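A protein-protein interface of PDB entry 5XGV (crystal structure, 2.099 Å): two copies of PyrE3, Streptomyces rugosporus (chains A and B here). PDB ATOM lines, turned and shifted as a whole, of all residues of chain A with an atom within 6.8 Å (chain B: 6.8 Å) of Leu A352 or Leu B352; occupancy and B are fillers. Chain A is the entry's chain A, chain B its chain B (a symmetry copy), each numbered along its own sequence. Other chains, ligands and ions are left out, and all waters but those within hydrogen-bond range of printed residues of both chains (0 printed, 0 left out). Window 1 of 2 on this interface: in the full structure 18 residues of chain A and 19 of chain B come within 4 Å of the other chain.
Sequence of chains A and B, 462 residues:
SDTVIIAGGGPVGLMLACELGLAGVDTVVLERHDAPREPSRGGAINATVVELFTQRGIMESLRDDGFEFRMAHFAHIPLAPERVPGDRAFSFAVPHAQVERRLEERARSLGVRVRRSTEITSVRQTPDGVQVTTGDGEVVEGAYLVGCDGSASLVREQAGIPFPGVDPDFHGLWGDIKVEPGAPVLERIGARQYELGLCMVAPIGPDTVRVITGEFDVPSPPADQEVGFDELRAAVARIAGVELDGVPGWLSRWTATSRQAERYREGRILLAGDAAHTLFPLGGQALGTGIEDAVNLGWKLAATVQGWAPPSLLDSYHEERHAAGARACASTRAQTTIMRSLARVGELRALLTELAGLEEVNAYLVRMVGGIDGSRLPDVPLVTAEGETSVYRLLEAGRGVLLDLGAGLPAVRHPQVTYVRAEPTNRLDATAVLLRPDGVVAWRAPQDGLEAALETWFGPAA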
ATOM      1  N   PHE A  74      21.050 -14.339  17.594  1.00  0.00           N
ATOM      2  CA  PHE A  74      20.763 -13.215  18.470  1.00  0.00           C
ATOM      3  C   PHE A  74      21.977 -13.013  19.396  1.00  0.00           C
ATOM      4  O   PHE A  74      22.188 -13.796  20.312  1.00  0.00           O
ATOM      5  CB  PHE A  74      19.488 -13.474  19.271  1.00  0.00           C
ATOM      6  CG  PHE A  74      19.118 -12.362  20.232  1.00  0.00           C
ATOM      7  CD1 PHE A  74      19.638 -12.331  21.517  1.00  0.00           C
ATOM      8  CD2 PHE A  74      18.220 -11.373  19.859  1.00  0.00           C
ATOM      9  CE1 PHE A  74      19.291 -11.324  22.406  1.00  0.00           C
ATOM     10  CE2 PHE A  74      17.854 -10.372  20.751  1.00  0.00           C
ATOM     11  CZ  PHE A  74      18.405 -10.342  22.021  1.00  0.00           C
ATOM     12  N   ILE A  77      24.016 -16.048  19.758  1.00  0.00           N
ATOM     13  CA  ILE A  77      23.254 -17.251  20.088  1.00  0.00           C
ATOM     14  C   ILE A  77      22.627 -17.784  18.801  1.00  0.00           C
ATOM     15  O   ILE A  77      21.810 -17.109  18.193  1.00  0.00           O
ATOM     16  CB  ILE A  77      22.138 -16.977  21.117  1.00  0.00           C
ATOM     17  CG1 ILE A  77      22.711 -16.353  22.391  1.00  0.00           C
ATOM     18  CG2 ILE A  77      21.321 -18.268  21.394  1.00  0.00           C
ATOM     19  CD1 ILE A  77      21.629 -15.864  23.359  1.00  0.00           C
ATOM     20  N   ALA A 334      19.453  -4.551  23.051  1.00  0.00           N
ATOM     21  CA  ALA A 334      19.184  -5.749  23.845  1.00  0.00           C
ATOM     22  C   ALA A 334      20.343  -6.704  23.594  1.00  0.00           C
ATOM     23  O   ALA A 334      20.999  -7.188  24.522  1.00  0.00           O
ATOM     24  CB  ALA A 334      17.838  -6.390  23.465  1.00  0.00           C
ATOM     25  N   ILE A 338      24.246  -8.247  26.035  1.00  0.00           N
ATOM     26  CA  ILE A 338      24.841  -9.526  26.395  1.00  0.00           C
ATOM     27  C   ILE A 338      26.033  -9.829  25.518  1.00  0.00           C
ATOM     28  O   ILE A 338      26.349 -10.989  25.294  1.00  0.00           O
ATOM     29  CB  ILE A 338      23.835 -10.709  26.304  1.00  0.00           C
ATOM     30  CG1 ILE A 338      23.141 -10.754  24.942  1.00  0.00           C
ATOM     31  CG2 ILE A 338      22.808 -10.622  27.428  1.00  0.00           C
ATOM     32  CD1 ILE A 338      22.287 -12.010  24.741  1.00  0.00           C
ATOM     33  N   GLU A 347      25.909 -16.238  32.366  1.00  0.00           N
ATOM     34  CA  GLU A 347      24.757 -16.968  32.880  1.00  0.00           C
ATOM     35  C   GLU A 347      23.477 -16.558  32.149  1.00  0.00           C
ATOM     36  O   GLU A 347      22.667 -17.404  31.787  1.00  0.00           O
ATOM     37  CB  GLU A 347      24.610 -16.766  34.394  1.00  0.00           C
ATOM     38  CG  GLU A 347      25.805 -17.286  35.227  1.00  0.00           C
ATOM     39  CD  GLU A 347      26.940 -16.262  35.350  1.00  0.00           C
ATOM     40  OE1 GLU A 347      26.810 -15.142  34.819  1.00  0.00           O
ATOM     41  OE2 GLU A 347      27.961 -16.575  35.980  1.00  0.00           O
ATOM     42  N   LEU A 348      23.311 -15.267  31.899  1.00  0.00           N
ATOM     43  CA  LEU A 348      22.123 -14.800  31.183  1.00  0.00           C
ATOM     44  C   LEU A 348      22.140 -15.271  29.734  1.00  0.00           C
ATOM     45  O   LEU A 348      21.093 -15.619  29.182  1.00  0.00           O
ATOM     46  CB  LEU A 348      22.000 -13.275  31.236  1.00  0.00           C
ATOM     47  CG  LEU A 348      20.722 -12.687  30.631  1.00  0.00           C
ATOM     48  CD1 LEU A 348      19.466 -13.300  31.279  1.00  0.00           C
ATOM     49  CD2 LEU A 348      20.701 -11.185  30.772  1.00  0.00           C
ATOM     50  N   ARG A 349      23.324 -15.281  29.119  1.00  0.00           N
ATOM     51  CA  ARG A 349      23.470 -15.815  27.762  1.00  0.00           C
ATOM     52  C   ARG A 349      23.048 -17.284  27.725  1.00  0.00           C
ATOM     53  O   ARG A 349      22.330 -17.690  26.820  1.00  0.00           O
ATOM     54  CB  ARG A 349      24.907 -15.675  27.245  1.00  0.00           C
ATOM     55  CG  ARG A 349      25.302 -14.273  26.795  1.00  0.00           C
ATOM     56  CD  ARG A 349      26.698 -14.266  26.159  1.00  0.00           C
ATOM     57  NE  ARG A 349      26.738 -15.033  24.917  1.00  0.00           N
ATOM     58  CZ  ARG A 349      26.321 -14.568  23.742  1.00  0.00           C
ATOM     59  NH1 ARG A 349      25.840 -13.324  23.647  1.00  0.00           N
ATOM     60  NH2 ARG A 349      26.381 -15.343  22.665  1.00  0.00           N
ATOM     61  N   ALA A 350      23.503 -18.073  28.701  1.00  0.00           N
ATOM     62  CA  ALA A 350      23.155 -19.500  28.760  1.00  0.00           C
ATOM     63  C   ALA A 350      21.648 -19.695  28.951  1.00  0.00           C
ATOM     64  O   ALA A 350      21.027 -20.549  28.305  1.00  0.00           O
ATOM     65  CB  ALA A 350      23.940 -20.211  29.884  1.00  0.00           C
ATOM     66  N   LEU A 351      21.062 -18.887  29.830  1.00  0.00           N
ATOM     67  CA  LEU A 351      19.624 -18.940  30.040  1.00  0.00           C
ATOM     68  C   LEU A 351      18.857 -18.638  28.738  1.00  0.00           C
ATOM     69  O   LEU A 351      17.969 -19.393  28.330  1.00  0.00           O
ATOM     70  CB  LEU A 351      19.216 -17.968  31.143  1.00  0.00           C
ATOM     71  CG  LEU A 351      17.711 -17.774  31.308  1.00  0.00           C
ATOM     72  CD1 LEU A 351      17.073 -19.081  31.676  1.00  0.00           C
ATOM     73  CD2 LEU A 351      17.447 -16.748  32.367  1.00  0.00           C
ATOM     74  N   LEU A 352      19.218 -17.543  28.082  1.00  0.00           N
ATOM     75  CA  LEU A 352      18.599 -17.169  26.815  1.00  0.00           C
ATOM     76  C   LEU A 352      18.788 -18.223  25.730  1.00  0.00           C
ATOM     77  O   LEU A 352      17.924 -18.407  24.868  1.00  0.00           O
ATOM     78  CB  LEU A 352      19.160 -15.839  26.320  1.00  0.00           C
ATOM     79  CG  LEU A 352      18.626 -14.605  27.041  1.00  0.00           C
ATOM     80  CD1 LEU A 352      19.452 -13.391  26.651  1.00  0.00           C
ATOM     81  CD2 LEU A 352      17.157 -14.413  26.657  1.00  0.00           C
ATOM     82  N   THR A 353      19.931 -18.888  25.762  1.00  0.00           N
ATOM     83  CA  THR A 353      20.206 -19.951  24.809  1.00  0.00           C
ATOM     84  C   THR A 353      19.235 -21.094  25.049  1.00  0.00           C
ATOM     85  O   THR A 353      18.688 -21.666  24.106  1.00  0.00           O
ATOM     86  CB  THR A 353      21.651 -20.448  24.917  1.00  0.00           C
ATOM     87  OG1 THR A 353      22.539 -19.366  24.648  1.00  0.00           O
ATOM     88  CG2 THR A 353      21.908 -21.594  23.940  1.00  0.00           C
ATOM     89  N   GLU A 354      18.992 -21.396  26.319  1.00  0.00           N
ATOM     90  CA  GLU A 354      18.003 -22.428  26.637  1.00  0.00           C
ATOM     91  C   GLU A 354      16.610 -21.997  26.177  1.00  0.00           C
ATOM     92  O   GLU A 354      15.892 -22.787  25.570  1.00  0.00           O
ATOM     93  CB  GLU A 354      18.007 -22.755  28.129  1.00  0.00           C
ATOM     94  CG  GLU A 354      19.271 -23.452  28.593  1.00  0.00           C
ATOM     95  CD  GLU A 354      19.802 -24.463  27.575  1.00  0.00           C
ATOM     96  OE1 GLU A 354      19.312 -25.611  27.580  1.00  0.00           O
ATOM     97  OE2 GLU A 354      20.716 -24.122  26.783  1.00  0.00           O
ATOM     98  N   LEU A 355      16.243 -20.740  26.419  1.00  0.00           N
ATOM     99  CA  LEU A 355      14.905 -20.282  26.047  1.00  0.00           C
ATOM    100  C   LEU A 355      14.717 -20.310  24.528  1.00  0.00           C
ATOM    101  O   LEU A 355      13.632 -20.609  24.042  1.00  0.00           O
ATOM    102  CB  LEU A 355      14.624 -18.879  26.591  1.00  0.00           C
ATOM    103  CG  LEU A 355      14.494 -18.697  28.112  1.00  0.00           C
ATOM    104  CD1 LEU A 355      14.236 -17.244  28.458  1.00  0.00           C
ATOM    105  CD2 LEU A 355      13.405 -19.572  28.693  1.00  0.00           C
ATOM    106  N   ALA A 356      15.783 -20.035  23.784  1.00  0.00           N
ATOM    107  CA  ALA A 356      15.702 -20.060  22.326  1.00  0.00           C
ATOM    108  C   ALA A 356      15.436 -21.473  21.770  1.00  0.00           C
ATOM    109  O   ALA A 356      15.141 -21.633  20.586  1.00  0.00           O
ATOM    110  CB  ALA A 356      16.971 -19.489  21.724  1.00  0.00           C
ATOM    111  N   GLY A 357      15.537 -22.485  22.627  1.00  0.00           N
ATOM    112  CA  GLY A 357      15.162 -23.841  22.262  1.00  0.00           C
ATOM    113  C   GLY A 357      13.651 -24.041  22.218  1.00  0.00           C
ATOM    114  O   GLY A 357      13.151 -24.996  21.610  1.00  0.00           O
ATOM    115  N   VAL A 361      10.004 -18.890  21.041  1.00  0.00           N
ATOM    116  CA  VAL A 361      11.112 -17.974  21.268  1.00  0.00           C
ATOM    117  C   VAL A 361      12.014 -17.936  20.042  1.00  0.00           C
ATOM    118  O   VAL A 361      12.413 -16.870  19.594  1.00  0.00           O
ATOM    119  CB  VAL A 361      11.940 -18.361  22.499  1.00  0.00           C
ATOM    120  CG1 VAL A 361      13.115 -17.407  22.675  1.00  0.00           C
ATOM    121  CG2 VAL A 361      11.072 -18.364  23.717  1.00  0.00           C
ATOM    122  N   LEU A 365      12.654 -14.507  17.930  1.00  0.00           N
ATOM    123  CA  LEU A 365      14.000 -13.979  17.716  1.00  0.00           C
ATOM    124  C   LEU A 365      14.423 -13.950  16.230  1.00  0.00           C
ATOM    125  O   LEU A 365      15.035 -12.980  15.772  1.00  0.00           O
ATOM    126  CB  LEU A 365      15.011 -14.779  18.537  1.00  0.00           C
ATOM    127  CG  LEU A 365      14.793 -14.656  20.044  1.00  0.00           C
ATOM    128  CD1 LEU A 365      15.802 -15.489  20.826  1.00  0.00           C
ATOM    129  CD2 LEU A 365      14.818 -13.187  20.492  1.00  0.00           C
ATOM    130  N   PHE B  74      11.088 -12.637  37.714  1.00  0.00           N
ATOM    131  CA  PHE B  74      12.469 -12.858  37.304  1.00  0.00           C
ATOM    132  C   PHE B  74      13.128 -11.478  37.201  1.00  0.00           C
ATOM    133  O   PHE B  74      12.808 -10.693  36.300  1.00  0.00           O
ATOM    134  CB  PHE B  74      12.536 -13.618  35.982  1.00  0.00           C
ATOM    135  CG  PHE B  74      13.935 -13.847  35.472  1.00  0.00           C
ATOM    136  CD1 PHE B  74      14.586 -12.870  34.743  1.00  0.00           C
ATOM    137  CD2 PHE B  74      14.582 -15.054  35.689  1.00  0.00           C
ATOM    138  CE1 PHE B  74      15.871 -13.080  34.263  1.00  0.00           C
ATOM    139  CE2 PHE B  74      15.863 -15.271  35.205  1.00  0.00           C
ATOM    140  CZ  PHE B  74      16.504 -14.278  34.497  1.00  0.00           C
ATOM    141  N   ILE B  77      10.674  -8.758  36.842  1.00  0.00           N
ATOM    142  CA  ILE B  77       9.710  -8.947  35.762  1.00  0.00           C
ATOM    143  C   ILE B  77       8.599  -9.869  36.262  1.00  0.00           C
ATOM    144  O   ILE B  77       8.870 -11.014  36.586  1.00  0.00           O
ATOM    145  CB  ILE B  77      10.370  -9.567  34.511  1.00  0.00           C
ATOM    146  CG1 ILE B  77      11.498  -8.654  34.003  1.00  0.00           C
ATOM    147  CG2 ILE B  77       9.323  -9.858  33.437  1.00  0.00           C
ATOM    148  CD1 ILE B  77      12.216  -9.195  32.791  1.00  0.00           C
ATOM    149  N   ALA B 334      21.997 -14.563  36.430  1.00  0.00           N
ATOM    150  CA  ALA B 334      21.281 -14.201  35.221  1.00  0.00           C
ATOM    151  C   ALA B 334      20.341 -13.060  35.557  1.00  0.00           C
ATOM    152  O   ALA B 334      20.223 -12.095  34.802  1.00  0.00           O
ATOM    153  CB  ALA B 334      20.500 -15.400  34.653  1.00  0.00           C
ATOM    154  N   ILE B 338      20.579  -8.180  34.827  1.00  0.00           N
ATOM    155  CA  ILE B 338      19.645  -7.157  34.348  1.00  0.00           C
ATOM    156  C   ILE B 338      19.006  -6.353  35.479  1.00  0.00           C
ATOM    157  O   ILE B 338      17.873  -5.903  35.348  1.00  0.00           O
ATOM    158  CB  ILE B 338      18.498  -7.750  33.480  1.00  0.00           C
ATOM    159  CG1 ILE B 338      17.783  -8.886  34.217  1.00  0.00           C
ATOM    160  CG2 ILE B 338      19.032  -8.249  32.144  1.00  0.00           C
ATOM    161  CD1 ILE B 338      16.538  -9.412  33.482  1.00  0.00           C
ATOM    162  N   GLU B 347      16.445  -2.147  27.607  1.00  0.00           N
ATOM    163  CA  GLU B 347      15.962  -2.753  26.367  1.00  0.00           C
ATOM    164  C   GLU B 347      15.891  -4.287  26.463  1.00  0.00           C
ATOM    165  O   GLU B 347      14.932  -4.917  25.990  1.00  0.00           O
ATOM    166  CB  GLU B 347      16.838  -2.329  25.186  1.00  0.00           C
ATOM    167  CG  GLU B 347      16.820  -0.825  24.898  1.00  0.00           C
ATOM    168  CD  GLU B 347      17.865  -0.076  25.698  1.00  0.00           C
ATOM    169  OE1 GLU B 347      18.555  -0.710  26.526  1.00  0.00           O
ATOM    170  OE2 GLU B 347      17.998   1.144  25.497  1.00  0.00           O
ATOM    171  N   LEU B 348      16.890  -4.886  27.095  1.00  0.00           N
ATOM    172  CA  LEU B 348      16.889  -6.329  27.257  1.00  0.00           C
ATOM    173  C   LEU B 348      15.797  -6.745  28.243  1.00  0.00           C
ATOM    174  O   LEU B 348      15.154  -7.785  28.064  1.00  0.00           O
ATOM    175  CB  LEU B 348      18.264  -6.835  27.715  1.00  0.00           C
ATOM    176  CG  LEU B 348      18.443  -8.350  27.918  1.00  0.00           C
ATOM    177  CD1 LEU B 348      18.113  -9.158  26.658  1.00  0.00           C
ATOM    178  CD2 LEU B 348      19.857  -8.636  28.342  1.00  0.00           C
ATOM    179  N   ARG B 349      15.585  -5.932  29.276  1.00  0.00           N
ATOM    180  CA  ARG B 349      14.492  -6.176  30.226  1.00  0.00           C
ATOM    181  C   ARG B 349      13.138  -6.176  29.513  1.00  0.00           C
ATOM    182  O   ARG B 349      12.310  -7.060  29.753  1.00  0.00           O
ATOM    183  CB  ARG B 349      14.497  -5.135  31.361  1.00  0.00           C
ATOM    184  CG  ARG B 349      15.623  -5.341  32.401  1.00  0.00           C
ATOM    185  CD  ARG B 349      15.507  -4.380  33.601  1.00  0.00           C
ATOM    186  NE  ARG B 349      14.245  -4.527  34.320  1.00  0.00           N
ATOM    187  CZ  ARG B 349      14.026  -5.456  35.244  1.00  0.00           C
ATOM    188  NH1 ARG B 349      14.988  -6.310  35.585  1.00  0.00           N
ATOM    189  NH2 ARG B 349      12.845  -5.538  35.815  1.00  0.00           N
ATOM    190  N   ALA B 350      12.929  -5.201  28.623  1.00  0.00           N
ATOM    191  CA  ALA B 350      11.675  -5.119  27.878  1.00  0.00           C
ATOM    192  C   ALA B 350      11.492  -6.324  26.947  1.00  0.00           C
ATOM    193  O   ALA B 350      10.397  -6.901  26.863  1.00  0.00           O
ATOM    194  CB  ALA B 350      11.603  -3.806  27.077  1.00  0.00           C
ATOM    195  N   LEU B 351      12.561  -6.693  26.246  1.00  0.00           N
ATOM    196  CA  LEU B 351      12.548  -7.907  25.431  1.00  0.00           C
ATOM    197  C   LEU B 351      12.167  -9.157  26.252  1.00  0.00           C
ATOM    198  O   LEU B 351      11.290  -9.917  25.870  1.00  0.00           O
ATOM    199  CB  LEU B 351      13.914  -8.108  24.764  1.00  0.00           C
ATOM    200  CG  LEU B 351      14.152  -9.456  24.078  1.00  0.00           C
ATOM    201  CD1 LEU B 351      13.110  -9.696  23.025  1.00  0.00           C
ATOM    202  CD2 LEU B 351      15.505  -9.456  23.453  1.00  0.00           C
ATOM    203  N   LEU B 352      12.830  -9.359  27.382  1.00  0.00           N
ATOM    204  CA  LEU B 352      12.520 -10.483  28.256  1.00  0.00           C
ATOM    205  C   LEU B 352      11.082 -10.466  28.785  1.00  0.00           C
ATOM    206  O   LEU B 352      10.500 -11.518  28.967  1.00  0.00           O
ATOM    207  CB  LEU B 352      13.499 -10.524  29.434  1.00  0.00           C
ATOM    208  CG  LEU B 352      14.819 -11.216  29.088  1.00  0.00           C
ATOM    209  CD1 LEU B 352      15.789 -11.204  30.263  1.00  0.00           C
ATOM    210  CD2 LEU B 352      14.551 -12.645  28.615  1.00  0.00           C
ATOM    211  N   THR B 353      10.536  -9.283  29.057  1.00  0.00           N
ATOM    212  CA  THR B 353       9.132  -9.146  29.461  1.00  0.00           C
ATOM    213  C   THR B 353       8.215  -9.661  28.349  1.00  0.00           C
ATOM    214  O   THR B 353       7.301 -10.484  28.586  1.00  0.00           O
ATOM    215  CB  THR B 353       8.800  -7.675  29.801  1.00  0.00           C
ATOM    216  OG1 THR B 353       9.658  -7.234  30.857  1.00  0.00           O
ATOM    217  CG2 THR B 353       7.323  -7.501  30.232  1.00  0.00           C
ATOM    218  N   GLU B 354       8.489  -9.201  27.127  1.00  0.00           N
ATOM    219  CA  GLU B 354       7.799  -9.727  25.947  1.00  0.00           C
ATOM    220  C   GLU B 354       7.878 -11.258  25.887  1.00  0.00           C
ATOM    221  O   GLU B 354       6.861 -11.932  25.732  1.00  0.00           O
ATOM    222  CB  GLU B 354       8.385  -9.140  24.667  1.00  0.00           C
ATOM    223  CG  GLU B 354       8.063  -7.684  24.427  1.00  0.00           C
ATOM    224  CD  GLU B 354       6.778  -7.505  23.656  1.00  0.00           C
ATOM    225  OE1 GLU B 354       6.829  -7.591  22.410  1.00  0.00           O
ATOM    226  OE2 GLU B 354       5.719  -7.293  24.294  1.00  0.00           O
ATOM    227  N   LEU B 355       9.088 -11.802  25.997  1.00  0.00           N
ATOM    228  CA  LEU B 355       9.272 -13.252  25.912  1.00  0.00           C
ATOM    229  C   LEU B 355       8.511 -13.984  27.014  1.00  0.00           C
ATOM    230  O   LEU B 355       7.920 -15.033  26.776  1.00  0.00           O
ATOM    231  CB  LEU B 355      10.759 -13.605  25.964  1.00  0.00           C
ATOM    232  CG  LEU B 355      11.550 -13.175  24.730  1.00  0.00           C
ATOM    233  CD1 LEU B 355      13.011 -13.561  24.845  1.00  0.00           C
ATOM    234  CD2 LEU B 355      10.930 -13.779  23.482  1.00  0.00           C
ATOM    235  N   ALA B 356       8.506 -13.409  28.209  1.00  0.00           N
ATOM    236  CA  ALA B 356       7.808 -13.984  29.349  1.00  0.00           C
ATOM    237  C   ALA B 356       6.306 -14.035  29.089  1.00  0.00           C
ATOM    238  O   ALA B 356       5.581 -14.778  29.754  1.00  0.00           O
ATOM    239  CB  ALA B 356       8.098 -13.199  30.617  1.00  0.00           C
ATOM    240  N   GLY B 357       5.844 -13.219  28.143  1.00  0.00           N
ATOM    241  CA  GLY B 357       4.488 -13.373  27.634  1.00  0.00           C
ATOM    242  C   GLY B 357       4.148 -14.719  26.982  1.00  0.00           C
ATOM    243  O   GLY B 357       2.978 -15.105  26.946  1.00  0.00           O
ATOM    244  N   VAL B 361       7.780 -19.862  28.188  1.00  0.00           N
ATOM    245  CA  VAL B 361       8.783 -19.053  28.871  1.00  0.00           C
ATOM    246  C   VAL B 361       8.335 -18.767  30.298  1.00  0.00           C
ATOM    247  O   VAL B 361       9.107 -18.944  31.240  1.00  0.00           O
ATOM    248  CB  VAL B 361       9.057 -17.724  28.137  1.00  0.00           C
ATOM    249  CG1 VAL B 361      10.011 -16.865  28.937  1.00  0.00           C
ATOM    250  CG2 VAL B 361       9.641 -18.001  26.792  1.00  0.00           C
ATOM    251  N   LEU B 365      10.409 -20.021  33.586  1.00  0.00           N
ATOM    252  CA  LEU B 365      10.909 -19.075  34.574  1.00  0.00           C
ATOM    253  C   LEU B 365      10.253 -19.243  35.951  1.00  0.00           C
ATOM    254  O   LEU B 365      10.926 -19.123  36.972  1.00  0.00           O
ATOM    255  CB  LEU B 365      10.725 -17.647  34.074  1.00  0.00           C
ATOM    256  CG  LEU B 365      11.541 -17.218  32.853  1.00  0.00           C
ATOM    257  CD1 LEU B 365      11.211 -15.783  32.462  1.00  0.00           C
ATOM    258  CD2 LEU B 365      13.055 -17.379  33.071  1.00  0.00           C
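O of Ile B338 lies within hydrogen-bond range of NH1 of Arg B349 (2.9 Å). The backbone carbonyl oxygen (O) of Ile A338 is in hydrogen-bond range of the guanidinium group (NH1) of Arg A349, 2.9 Å away.
Phe A74 touches Leu B351, and with the chains exchanged Leu A351 touches Phe B74. Glu A347 touches Ala B334, but with the chains exchanged Ala A334 does not touch Glu B347 (4.04 Å). Leu A348 touches its own counterpart, Leu B348. Val A361 touches its own counterpart, Val B361. 17 positions are printed for both chains.
Hydrophobic or aromatic side chains of chain B that line the printed part of chain A: Phe B74, Ala B334, Ile B338, Leu B348, Leu B351, Leu B352 and Val B361. Hydrophobic or aromatic side chains of chain A within 4 Å of the printed part of chain B: Phe A74, Ala A334, Ile A338, Leu A348, Leu A351, Leu A352 and Val A361.
Of chain B, only Leu B352 (3.7 Å) comes within 4 Å of Leu A352. Of chain A, only Leu A352 (3.7 Å) comes within 4 Å of Leu B352. Of the printed residues of chain A, Ala B334 touches Glu A347 (3.98 Å) and Leu A348 (3.8 Å). Printed residues of chain A within 4 Å of Ile B338: Leu A348 (3.6 Å). The nearest residue of chain B that does not touch Leu A352 is Leu B348 (4.4 Å).
Among the printed residues, pairs that only touch across the chains: Phe A74 with Leu B351, Leu A351 with Phe B74, Val A361 with Val B361, Leu A348 with Leu B348, Leu A348 with Ile B338, Ile A338 with Leu B348, Leu A352 with Leu B352, Leu A348 with Ala B334, Ala A334 with Leu B351, Ala A334 with Leu B348 and Glu A347 with Ala B334.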
